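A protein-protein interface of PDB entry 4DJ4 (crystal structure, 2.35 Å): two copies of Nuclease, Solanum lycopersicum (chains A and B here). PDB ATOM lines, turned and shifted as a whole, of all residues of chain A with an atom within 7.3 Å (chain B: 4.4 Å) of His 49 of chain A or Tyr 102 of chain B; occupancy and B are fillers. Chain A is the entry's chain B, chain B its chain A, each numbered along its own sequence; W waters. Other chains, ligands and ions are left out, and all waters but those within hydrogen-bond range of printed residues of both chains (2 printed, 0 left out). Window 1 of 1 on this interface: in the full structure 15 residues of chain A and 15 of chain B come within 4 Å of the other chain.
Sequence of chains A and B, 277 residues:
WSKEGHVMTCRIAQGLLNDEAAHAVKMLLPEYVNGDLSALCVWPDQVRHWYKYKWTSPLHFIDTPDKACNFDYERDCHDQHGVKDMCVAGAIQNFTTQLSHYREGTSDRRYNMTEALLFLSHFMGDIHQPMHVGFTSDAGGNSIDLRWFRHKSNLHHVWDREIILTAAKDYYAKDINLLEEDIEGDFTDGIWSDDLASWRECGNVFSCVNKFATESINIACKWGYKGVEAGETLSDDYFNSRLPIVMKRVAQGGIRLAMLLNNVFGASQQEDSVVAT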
ATOM      1  N   PRO A  44      22.719 -17.138  -7.409  1.00  0.00           N
ATOM      2  CA  PRO A  44      21.771 -16.105  -6.942  1.00  0.00           C
ATOM      3  C   PRO A  44      20.548 -16.585  -6.168  1.00  0.00           C
ATOM      4  O   PRO A  44      19.936 -15.782  -5.446  1.00  0.00           O
ATOM      5  CB  PRO A  44      21.314 -15.453  -8.247  1.00  0.00           C
ATOM      6  CG  PRO A  44      22.547 -15.553  -9.096  1.00  0.00           C
ATOM      7  CD  PRO A  44      22.990 -16.976  -8.843  1.00  0.00           C
ATOM      8  N   ASP A  45      20.164 -17.849  -6.347  1.00  0.00           N
ATOM      9  CA  ASP A  45      18.965 -18.393  -5.682  1.00  0.00           C
ATOM     10  C   ASP A  45      19.316 -18.801  -4.250  1.00  0.00           C
ATOM     11  O   ASP A  45      18.456 -18.761  -3.374  1.00  0.00           O
ATOM     12  CB  ASP A  45      18.300 -19.534  -6.489  1.00  0.00           C
ATOM     13  CG  ASP A  45      17.194 -19.015  -7.481  1.00  0.00           C
ATOM     14  OD1 ASP A  45      16.619 -17.933  -7.246  1.00  0.00           O
ATOM     15  OD2 ASP A  45      16.886 -19.685  -8.494  1.00  0.00           O
ATOM     16  N   GLN A  46      20.581 -19.141  -3.999  1.00  0.00           N
ATOM     17  CA  GLN A  46      21.058 -19.298  -2.615  1.00  0.00           C
ATOM     18  C   GLN A  46      21.187 -17.929  -1.936  1.00  0.00           C
ATOM     19  O   GLN A  46      20.573 -17.683  -0.868  1.00  0.00           O
ATOM     20  CB  GLN A  46      22.394 -20.043  -2.550  1.00  0.00           C
ATOM     21  CG  GLN A  46      22.323 -21.539  -2.854  1.00  0.00           C
ATOM     22  CD  GLN A  46      22.854 -21.916  -4.238  1.00  0.00           C
ATOM     23  OE1 GLN A  46      24.060 -21.790  -4.524  1.00  0.00           O
ATOM     24  NE2 GLN A  46      21.957 -22.408  -5.100  1.00  0.00           N
ATOM     25  N   VAL A  47      21.934 -17.019  -2.576  1.00  0.00           N
ATOM     26  CA  VAL A  47      22.381 -15.778  -1.891  1.00  0.00           C
ATOM     27  C   VAL A  47      21.244 -14.802  -1.627  1.00  0.00           C
ATOM     28  O   VAL A  47      21.383 -13.915  -0.776  1.00  0.00           O
ATOM     29  CB  VAL A  47      23.584 -15.050  -2.604  1.00  0.00           C
ATOM     30  CG1 VAL A  47      24.668 -16.034  -3.019  1.00  0.00           C
ATOM     31  CG2 VAL A  47      23.127 -14.255  -3.806  1.00  0.00           C
ATOM     32  N   ARG A  48      20.117 -14.965  -2.311  1.00  0.00           N
ATOM     33  CA  ARG A  48      18.952 -14.091  -2.078  1.00  0.00           C
ATOM     34  C   ARG A  48      18.367 -14.217  -0.661  1.00  0.00           C
ATOM     35  O   ARG A  48      17.590 -13.373  -0.240  1.00  0.00           O
ATOM     36  CB  ARG A  48      17.832 -14.365  -3.106  1.00  0.00           C
ATOM     37  CG  ARG A  48      17.131 -15.718  -2.920  1.00  0.00           C
ATOM     38  CD  ARG A  48      16.028 -16.017  -3.944  1.00  0.00           C
ATOM     39  NE  ARG A  48      14.910 -15.076  -3.861  1.00  0.00           N
ATOM     40  CZ  ARG A  48      13.913 -14.986  -4.749  1.00  0.00           C
ATOM     41  NH1 ARG A  48      13.857 -15.797  -5.814  1.00  0.00           N
ATOM     42  NH2 ARG A  48      12.957 -14.072  -4.575  1.00  0.00           N
ATOM     43  N   HIS A  49      18.695 -15.296   0.042  1.00  0.00           N
ATOM     44  CA  HIS A  49      18.252 -15.496   1.417  1.00  0.00           C
ATOM     45  C   HIS A  49      19.247 -15.014   2.423  1.00  0.00           C
ATOM     46  O   HIS A  49      18.919 -14.927   3.607  1.00  0.00           O
ATOM     47  CB  HIS A  49      17.998 -16.977   1.677  1.00  0.00           C
ATOM     48  CG  HIS A  49      17.010 -17.592   0.730  1.00  0.00           C
ATOM     49  ND1 HIS A  49      15.690 -17.262   0.744  1.00  0.00           N
ATOM     50  CD2 HIS A  49      17.179 -18.542  -0.291  1.00  0.00           C
ATOM     51  CE1 HIS A  49      15.049 -17.946  -0.246  1.00  0.00           C
ATOM     52  NE2 HIS A  49      15.956 -18.738  -0.867  1.00  0.00           N
ATOM     53  N   TRP A  50      20.470 -14.714   1.980  1.00  0.00           N
ATOM     54  CA  TRP A  50      21.533 -14.191   2.862  1.00  0.00           C
ATOM     55  C   TRP A  50      21.201 -12.798   3.265  1.00  0.00           C
ATOM     56  O   TRP A  50      20.705 -12.037   2.436  1.00  0.00           O
ATOM     57  CB  TRP A  50      22.873 -14.201   2.137  1.00  0.00           C
ATOM     58  CG  TRP A  50      23.369 -15.579   1.807  1.00  0.00           C
ATOM     59  CD1 TRP A  50      22.664 -16.772   1.878  1.00  0.00           C
ATOM     60  CD2 TRP A  50      24.702 -15.957   1.303  1.00  0.00           C
ATOM     61  NE1 TRP A  50      23.446 -17.828   1.505  1.00  0.00           N
ATOM     62  CE2 TRP A  50      24.677 -17.414   1.145  1.00  0.00           C
ATOM     63  CE3 TRP A  50      25.869 -15.265   1.007  1.00  0.00           C
ATOM     64  CZ2 TRP A  50      25.777 -18.129   0.688  1.00  0.00           C
ATOM     65  CZ3 TRP A  50      26.980 -15.992   0.570  1.00  0.00           C
ATOM     66  CH2 TRP A  50      26.933 -17.397   0.409  1.00  0.00           C
ATOM     67  N   TYR A  51      21.455 -12.429   4.530  1.00  0.00           N
ATOM     68  CA  TYR A  51      21.234 -11.030   4.989  1.00  0.00           C
ATOM     69  C   TYR A  51      21.983 -10.004   4.112  1.00  0.00           C
ATOM     70  O   TYR A  51      21.462  -8.917   3.799  1.00  0.00           O
ATOM     71  CB  TYR A  51      21.701 -10.850   6.445  1.00  0.00           C
ATOM     72  CG  TYR A  51      21.694  -9.409   6.914  1.00  0.00           C
ATOM     73  CD1 TYR A  51      20.506  -8.803   7.346  1.00  0.00           C
ATOM     74  CD2 TYR A  51      22.866  -8.643   6.918  1.00  0.00           C
ATOM     75  CE1 TYR A  51      20.482  -7.472   7.770  1.00  0.00           C
ATOM     76  CE2 TYR A  51      22.853  -7.305   7.328  1.00  0.00           C
ATOM     77  CZ  TYR A  51      21.656  -6.727   7.753  1.00  0.00           C
ATOM     78  OH  TYR A  51      21.628  -5.407   8.166  1.00  0.00           O
ATOM     79  N   LYS A  52      23.234 -10.351   3.792  1.00  0.00           N
ATOM     80  CA  LYS A  52      24.144  -9.503   3.011  1.00  0.00           C
ATOM     81  C   LYS A  52      23.577  -9.122   1.621  1.00  0.00           C
ATOM     82  O   LYS A  52      23.881  -8.050   1.107  1.00  0.00           O
ATOM     83  CB  LYS A  52      25.475 -10.256   2.869  1.00  0.00           C
ATOM     84  CG  LYS A  52      26.605  -9.566   2.114  1.00  0.00           C
ATOM     85  CD  LYS A  52      27.963 -10.182   2.509  1.00  0.00           C
ATOM     86  CE  LYS A  52      28.898 -10.465   1.329  1.00  0.00           C
ATOM     87  NZ  LYS A  52      29.525  -9.258   0.721  1.00  0.00           N
ATOM     88  N   TYR A  53      22.750 -10.003   1.041  1.00  0.00           N
ATOM     89  CA  TYR A  53      22.167  -9.811  -0.295  1.00  0.00           C
ATOM     90  C   TYR A  53      20.639  -9.778  -0.320  1.00  0.00           C
ATOM     91  O   TYR A  53      20.036 -10.125  -1.340  1.00  0.00           O
ATOM     92  CB  TYR A  53      22.611 -10.946  -1.200  1.00  0.00           C
ATOM     93  CG  TYR A  53      24.092 -11.039  -1.403  1.00  0.00           C
ATOM     94  CD1 TYR A  53      24.725 -10.321  -2.414  1.00  0.00           C
ATOM     95  CD2 TYR A  53      24.859 -11.870  -0.609  1.00  0.00           C
ATOM     96  CE1 TYR A  53      26.090 -10.417  -2.610  1.00  0.00           C
ATOM     97  CE2 TYR A  53      26.220 -11.970  -0.781  1.00  0.00           C
ATOM     98  CZ  TYR A  53      26.836 -11.250  -1.787  1.00  0.00           C
ATOM     99  OH  TYR A  53      28.192 -11.387  -1.952  1.00  0.00           O
ATOM    100  N   LYS A  54      20.008  -9.378   0.787  1.00  0.00           N
ATOM    101  CA  LYS A  54      18.533  -9.241   0.834  1.00  0.00           C
ATOM    102  C   LYS A  54      17.991  -8.495  -0.367  1.00  0.00           C
ATOM    103  O   LYS A  54      16.964  -8.860  -0.904  1.00  0.00           O
ATOM    104  CB  LYS A  54      18.078  -8.427   2.047  1.00  0.00           C
ATOM    105  CG  LYS A  54      18.016  -9.119   3.384  1.00  0.00           C
ATOM    106  CD  LYS A  54      17.060  -8.333   4.287  1.00  0.00           C
ATOM    107  CE  LYS A  54      17.260  -8.631   5.754  1.00  0.00           C
ATOM    108  NZ  LYS A  54      16.056  -8.260   6.552  1.00  0.00           N
ATOM    109  N   THR A  56      18.822  -8.394  -3.352  1.00  0.00           N
ATOM    110  CA  THR A  56      18.733  -9.124  -4.611  1.00  0.00           C
ATOM    111  C   THR A  56      17.372  -9.802  -4.766  1.00  0.00           C
ATOM    112  O   THR A  56      16.958 -10.109  -5.882  1.00  0.00           O
ATOM    113  CB  THR A  56      19.846 -10.175  -4.741  1.00  0.00           C
ATOM    114  OG1 THR A  56      19.636 -11.210  -3.772  1.00  0.00           O
ATOM    115  CG2 THR A  56      21.259  -9.527  -4.546  1.00  0.00           C
ATOM    116  N   SER A  57      16.665  -9.990  -3.660  1.00  0.00           N
ATOM    117  CA  SER A  57      15.376 -10.700  -3.670  1.00  0.00           C
ATOM    118  C   SER A  57      14.416 -10.315  -4.799  1.00  0.00           C
ATOM    119  O   SER A  57      14.029 -11.181  -5.581  1.00  0.00           O
ATOM    120  CB  SER A  57      14.675 -10.639  -2.313  1.00  0.00           C
ATOM    121  OG  SER A  57      13.661 -11.629  -2.283  1.00  0.00           O
ATOM    122  N   HIS A  60      14.757 -11.149  -9.062  1.00  0.00           N
ATOM    123  CA  HIS A  60      14.463 -12.440  -9.709  1.00  0.00           C
ATOM    124  C   HIS A  60      13.240 -12.368 -10.606  1.00  0.00           C
ATOM    125  O   HIS A  60      13.081 -13.217 -11.499  1.00  0.00           O
ATOM    126  CB  HIS A  60      14.354 -13.545  -8.641  1.00  0.00           C
ATOM    127  CG  HIS A  60      15.679 -13.828  -7.984  1.00  0.00           C
ATOM    128  ND1 HIS A  60      16.476 -14.834  -8.374  1.00  0.00           N
ATOM    129  CD2 HIS A  60      16.400 -13.102  -7.028  1.00  0.00           C
ATOM    130  CE1 HIS A  60      17.632 -14.795  -7.672  1.00  0.00           C
ATOM    131  NE2 HIS A  60      17.585 -13.728  -6.846  1.00  0.00           N
ATOM    132  N   ALA B  24      25.835 -21.844   6.673  1.00  0.00           N
ATOM    133  CA  ALA B  24      24.458 -21.482   6.274  1.00  0.00           C
ATOM    134  C   ALA B  24      23.799 -20.594   7.346  1.00  0.00           C
ATOM    135  O   ALA B  24      23.190 -19.544   7.052  1.00  0.00           O
ATOM    136  CB  ALA B  24      23.602 -22.741   6.010  1.00  0.00           C
ATOM    137  N   LEU B  28      22.426 -16.858   7.065  1.00  0.00           N
ATOM    138  CA  LEU B  28      20.990 -16.583   7.251  1.00  0.00           C
ATOM    139  C   LEU B  28      20.663 -15.557   8.347  1.00  0.00           C
ATOM    140  O   LEU B  28      19.573 -15.016   8.346  1.00  0.00           O
ATOM    141  CB  LEU B  28      20.255 -17.883   7.505  1.00  0.00           C
ATOM    142  CG  LEU B  28      20.137 -18.803   6.286  1.00  0.00           C
ATOM    143  CD1 LEU B  28      19.546 -20.149   6.717  1.00  0.00           C
ATOM    144  CD2 LEU B  28      19.293 -18.127   5.214  1.00  0.00           C
ATOM    145  N   GLN B  98      11.397 -26.892   4.010  1.00  0.00           N
ATOM    146  CA  GLN B  98      11.818 -25.583   3.441  1.00  0.00           C
ATOM    147  C   GLN B  98      13.333 -25.361   3.405  1.00  0.00           C
ATOM    148  O   GLN B  98      13.880 -24.909   2.416  1.00  0.00           O
ATOM    149  CB  GLN B  98      11.198 -24.441   4.208  1.00  0.00           C
ATOM    150  CG  GLN B  98       9.682 -24.428   4.141  1.00  0.00           C
ATOM    151  CD  GLN B  98       9.135 -23.153   4.688  1.00  0.00           C
ATOM    152  OE1 GLN B  98       9.831 -22.141   4.676  1.00  0.00           O
ATOM    153  NE2 GLN B  98       7.895 -23.177   5.174  1.00  0.00           N
ATOM    154  N   LEU B  99      14.016 -25.712   4.480  1.00  0.00           N
ATOM    155  CA  LEU B  99      15.456 -25.562   4.522  1.00  0.00           C
ATOM    156  C   LEU B  99      16.219 -26.529   3.574  1.00  0.00           C
ATOM    157  O   LEU B  99      17.362 -26.240   3.147  1.00  0.00           O
ATOM    158  CB  LEU B  99      15.932 -25.726   5.976  1.00  0.00           C
ATOM    159  CG  LEU B  99      15.694 -24.524   6.899  1.00  0.00           C
ATOM    160  CD1 LEU B  99      16.192 -24.810   8.329  1.00  0.00           C
ATOM    161  CD2 LEU B  99      16.399 -23.297   6.315  1.00  0.00           C
ATOM    162  N   SER B 100      15.609 -27.680   3.278  1.00  0.00           N
ATOM    163  CA  SER B 100      16.223 -28.670   2.381  1.00  0.00           C
ATOM    164  C   SER B 100      16.257 -28.140   0.945  1.00  0.00           C
ATOM    165  O   SER B 100      17.145 -28.498   0.179  1.00  0.00           O
ATOM    166  CB  SER B 100      15.499 -30.033   2.450  1.00  0.00           C
ATOM    167  OG  SER B 100      14.134 -29.934   2.043  1.00  0.00           O
ATOM    168  N   HIS B 101      15.291 -27.284   0.610  1.00  0.00           N
ATOM    169  CA  HIS B 101      15.276 -26.533  -0.649  1.00  0.00           C
ATOM    170  C   HIS B 101      16.368 -25.500  -0.779  1.00  0.00           C
ATOM    171  O   HIS B 101      16.900 -25.293  -1.871  1.00  0.00           O
ATOM    172  CB  HIS B 101      13.943 -25.817  -0.841  1.00  0.00           C
ATOM    173  CG  HIS B 101      12.763 -26.743  -1.048  1.00  0.00           C
ATOM    174  ND1 HIS B 101      12.811 -27.806  -1.870  1.00  0.00           N
ATOM    175  CD2 HIS B 101      11.464 -26.701  -0.537  1.00  0.00           C
ATOM    176  CE1 HIS B 101      11.619 -28.433  -1.863  1.00  0.00           C
ATOM    177  NE2 HIS B 101      10.795 -27.752  -1.052  1.00  0.00           N
ATOM    178  N   TYR B 102      16.712 -24.828   0.312  1.00  0.00           N
ATOM    179  CA  TYR B 102      17.757 -23.799   0.272  1.00  0.00           C
ATOM    180  C   TYR B 102      19.054 -24.386  -0.285  1.00  0.00           C
ATOM    181  O   TYR B 102      19.708 -23.775  -1.157  1.00  0.00           O
ATOM    182  CB  TYR B 102      17.964 -23.199   1.679  1.00  0.00           C
ATOM    183  CG  TYR B 102      19.237 -22.405   1.895  1.00  0.00           C
ATOM    184  CD1 TYR B 102      19.312 -21.043   1.564  1.00  0.00           C
ATOM    185  CD2 TYR B 102      20.365 -23.011   2.444  1.00  0.00           C
ATOM    186  CE1 TYR B 102      20.481 -20.315   1.770  1.00  0.00           C
ATOM    187  CE2 TYR B 102      21.537 -22.299   2.652  1.00  0.00           C
ATOM    188  CZ  TYR B 102      21.594 -20.951   2.319  1.00  0.00           C
ATOM    189  OH  TYR B 102      22.773 -20.263   2.534  1.00  0.00           O
ATOM    190  N   ARG B 103      19.401 -25.582   0.201  1.00  0.00           N
ATOM    191  CA  ARG B 103      20.687 -26.226  -0.120  1.00  0.00           C
ATOM    192  C   ARG B 103      20.925 -26.353  -1.636  1.00  0.00           C
ATOM    193  O   ARG B 103      22.025 -26.065  -2.122  1.00  0.00           O
ATOM    194  CB  ARG B 103      20.769 -27.603   0.554  1.00  0.00           C
ATOM    195  CG  ARG B 103      22.129 -28.265   0.461  1.00  0.00           C
ATOM    196  CD  ARG B 103      22.035 -29.733   0.824  1.00  0.00           C
ATOM    197  NE  ARG B 103      23.132 -30.500   0.243  1.00  0.00           N
ATOM    198  CZ  ARG B 103      23.036 -31.178  -0.897  1.00  0.00           C
ATOM    199  NH1 ARG B 103      21.893 -31.180  -1.575  1.00  0.00           N
ATOM    200  NH2 ARG B 103      24.079 -31.852  -1.362  1.00  0.00           N
ATOM    201  N   GLU B 104      19.892 -26.778  -2.367  1.00  0.00           N
ATOM    202  CA  GLU B 104      19.937 -26.890  -3.839  1.00  0.00           C
ATOM    203  C   GLU B 104      19.588 -25.563  -4.518  1.00  0.00           C
ATOM    204  O   GLU B 104      19.985 -25.317  -5.654  1.00  0.00           O
ATOM    205  CB  GLU B 104      18.958 -27.969  -4.312  1.00  0.00           C
ATOM    206  CG  GLU B 104      19.218 -29.348  -3.723  1.00  0.00           C
ATOM    207  CD  GLU B 104      17.940 -30.088  -3.369  1.00  0.00           C
ATOM    208  OE1 GLU B 104      16.888 -29.807  -3.984  1.00  0.00           O
ATOM    209  OE2 GLU B 104      17.987 -30.956  -2.471  1.00  0.00           O
ATOM    210  N   GLY B 105      18.835 -24.716  -3.816  1.00  0.00           N
ATOM    211  CA  GLY B 105      18.332 -23.452  -4.361  1.00  0.00           C
ATOM    212  C   GLY B 105      16.880 -23.568  -4.781  1.00  0.00           C
ATOM    213  O   GLY B 105      16.130 -22.596  -4.691  1.00  0.00           O
ATOM    214  N   SER B 107      13.600 -23.480  -4.880  1.00  0.00           N
ATOM    215  CA  SER B 107      12.383 -22.998  -4.216  1.00  0.00           C
ATOM    216  C   SER B 107      12.030 -21.638  -4.817  1.00  0.00           C
ATOM    217  O   SER B 107      12.688 -21.199  -5.762  1.00  0.00           O
ATOM    218  CB  SER B 107      12.617 -22.873  -2.702  1.00  0.00           C
ATOM    219  OG  SER B 107      13.845 -22.204  -2.411  1.00  0.00           O
ATOM    220  N   TYR B 111       8.977 -18.863   0.491  1.00  0.00           N
ATOM    221  CA  TYR B 111       9.738 -19.188   1.702  1.00  0.00           C
ATOM    222  C   TYR B 111      10.928 -18.271   1.996  1.00  0.00           C
ATOM    223  O   TYR B 111      11.784 -18.016   1.154  1.00  0.00           O
ATOM    224  CB  TYR B 111      10.245 -20.623   1.640  1.00  0.00           C
ATOM    225  CG  TYR B 111       9.166 -21.667   1.451  1.00  0.00           C
ATOM    226  CD1 TYR B 111       9.394 -22.785   0.664  1.00  0.00           C
ATOM    227  CD2 TYR B 111       7.931 -21.543   2.066  1.00  0.00           C
ATOM    228  CE1 TYR B 111       8.420 -23.753   0.492  1.00  0.00           C
ATOM    229  CE2 TYR B 111       6.946 -22.501   1.891  1.00  0.00           C
ATOM    230  CZ  TYR B 111       7.201 -23.603   1.103  1.00  0.00           C
ATOM    231  OH  TYR B 111       6.233 -24.563   0.930  1.00  0.00           O
ATOM    232  N   MET B 113      14.101 -18.121   4.295  1.00  0.00           N
ATOM    233  CA  MET B 113      14.916 -19.129   4.967  1.00  0.00           C
ATOM    234  C   MET B 113      15.429 -18.684   6.322  1.00  0.00           C
ATOM    235  O   MET B 113      15.689 -19.525   7.176  1.00  0.00           O
ATOM    236  CB  MET B 113      16.083 -19.558   4.093  1.00  0.00           C
ATOM    237  CG  MET B 113      15.633 -20.254   2.829  1.00  0.00           C
ATOM    238  SD  MET B 113      14.659 -21.759   3.123  1.00  0.00           S
ATOM    239  CE  MET B 113      14.130 -22.092   1.429  1.00  0.00           C
ATOM    240  N   THR B 114      15.552 -17.370   6.520  1.00  0.00           N
ATOM    241  CA  THR B 114      15.849 -16.818   7.842  1.00  0.00           C
ATOM    242  C   THR B 114      14.693 -17.143   8.783  1.00  0.00           C
ATOM    243  O   THR B 114      14.890 -17.638   9.890  1.00  0.00           O
ATOM    244  CB  THR B 114      16.087 -15.294   7.797  1.00  0.00           C
ATOM    245  OG1 THR B 114      17.277 -15.025   7.049  1.00  0.00           O
ATOM    246  CG2 THR B 114      16.221 -14.723   9.217  1.00  0.00           C
ATOM    247  N   PHE B 265      21.563 -29.074   5.696  1.00  0.00           N
ATOM    248  CA  PHE B 265      22.536 -28.260   4.957  1.00  0.00           C
ATOM    249  C   PHE B 265      23.698 -29.083   4.421  1.00  0.00           C
ATOM    250  O   PHE B 265      24.045 -28.958   3.249  1.00  0.00           O
ATOM    251  CB  PHE B 265      23.077 -27.115   5.824  1.00  0.00           C
ATOM    252  CG  PHE B 265      22.038 -26.091   6.198  1.00  0.00           C
ATOM    253  CD1 PHE B 265      21.289 -25.454   5.227  1.00  0.00           C
ATOM    254  CD2 PHE B 265      21.834 -25.743   7.522  1.00  0.00           C
ATOM    255  CE1 PHE B 265      20.335 -24.512   5.575  1.00  0.00           C
ATOM    256  CE2 PHE B 265      20.893 -24.793   7.869  1.00  0.00           C
ATOM    257  CZ  PHE B 265      20.142 -24.179   6.892  1.00  0.00           C
HETATM  258  O   HOH W   1      15.983 -15.483   4.401  1.00  0.00           O
HETATM  259  O   HOH W   2      16.729 -12.539   4.748  1.00  0.00           O
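Water W1 lies within hydrogen-bond range of the backbone NH of Thr 114 of chain B, the backbone carbonyl oxygen of His 49 of chain A and the backbone NH of Met 113 of chain B. Water W2 bridges the side-chain hydroxyl of Thr 114 of chain B (3.4 Å) and the backbone carbonyl oxygen of His 49 of chain A (3.4 Å).
The side-chain hydroxyl of Tyr 102 of chain B lies within hydrogen-bond range of the indole nitrogen of Trp 50 of chain A (2.7 Å).
Among the printed residues, pairs that only touch across the chains: His 49 of chain A with Tyr 111 of chain B (3.6 Å), Gln 46 of chain A with Glu 104 of chain B (3.6 Å), His 49 of chain A with Leu 28 of chain B (3.6 Å), His 49 of chain A with Met 113 of chain B (3.6 Å), Gln 46 of chain A with Tyr 102 of chain B (3.7 Å), His 49 of chain A with Tyr 102 of chain B (3.8 Å), His 49 of chain A with Thr 114 of chain B (3.8 Å) and Gln 46 of chain A with Gly 105 of chain B (3.8 Å).
Of the 14 printed residues of chain A, 3 touch a printed residue of chain B. Printed residues of chain A that touch a printed residue of chain B: Gln 46, His 49 and Trp 50. Hydrophobic or aromatic side chains of chain A within 4 Å of the printed part of chain B: His 49 and Trp 50. Printed residues of chain B that touch a printed residue of chain A: Leu 28, Tyr 102, Glu 104, Gly 105, Tyr 111, Met 113 and Thr 114. Hydrophobic or aromatic side chains of chain B within 4 Å of the printed part of chain A: Leu 28, Tyr 102 and Met 113.
The side-chain hydroxyl of Thr 114 of chain B is in hydrogen-bond range of the backbone carbonyl oxygen of Leu 28 of chain B, at 2.6 Å. The backbone carbonyl oxygen (O) of Gly 105 of chain B is in hydrogen-bond range of the side-chain hydroxyl (OG) of Ser 107 of chain B (3.3 Å).
No position is printed for both chains.
His 49 of chain A touches five residues of chain B. Tyr 102 of chain B touches just these residues of chain A: Gln 46, His 49 and Trp 50. Printed residues of chain A within 4 Å of Thr 114 of chain B: His 49 (3.8 Å). Of the printed residues of chain A, Glu 104 of chain B touches Gln 46 (3.6 Å). Lys 54 of chain A touches none of the printed residues of chain B. The nearest residue of chain B that does not touch His 49 of chain A is Ser 107 of chain B (4.3 Å). The nearest residue of chain A that does not touch Tyr 102 of chain B is Asp 45 of chain A (5.5 Å).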
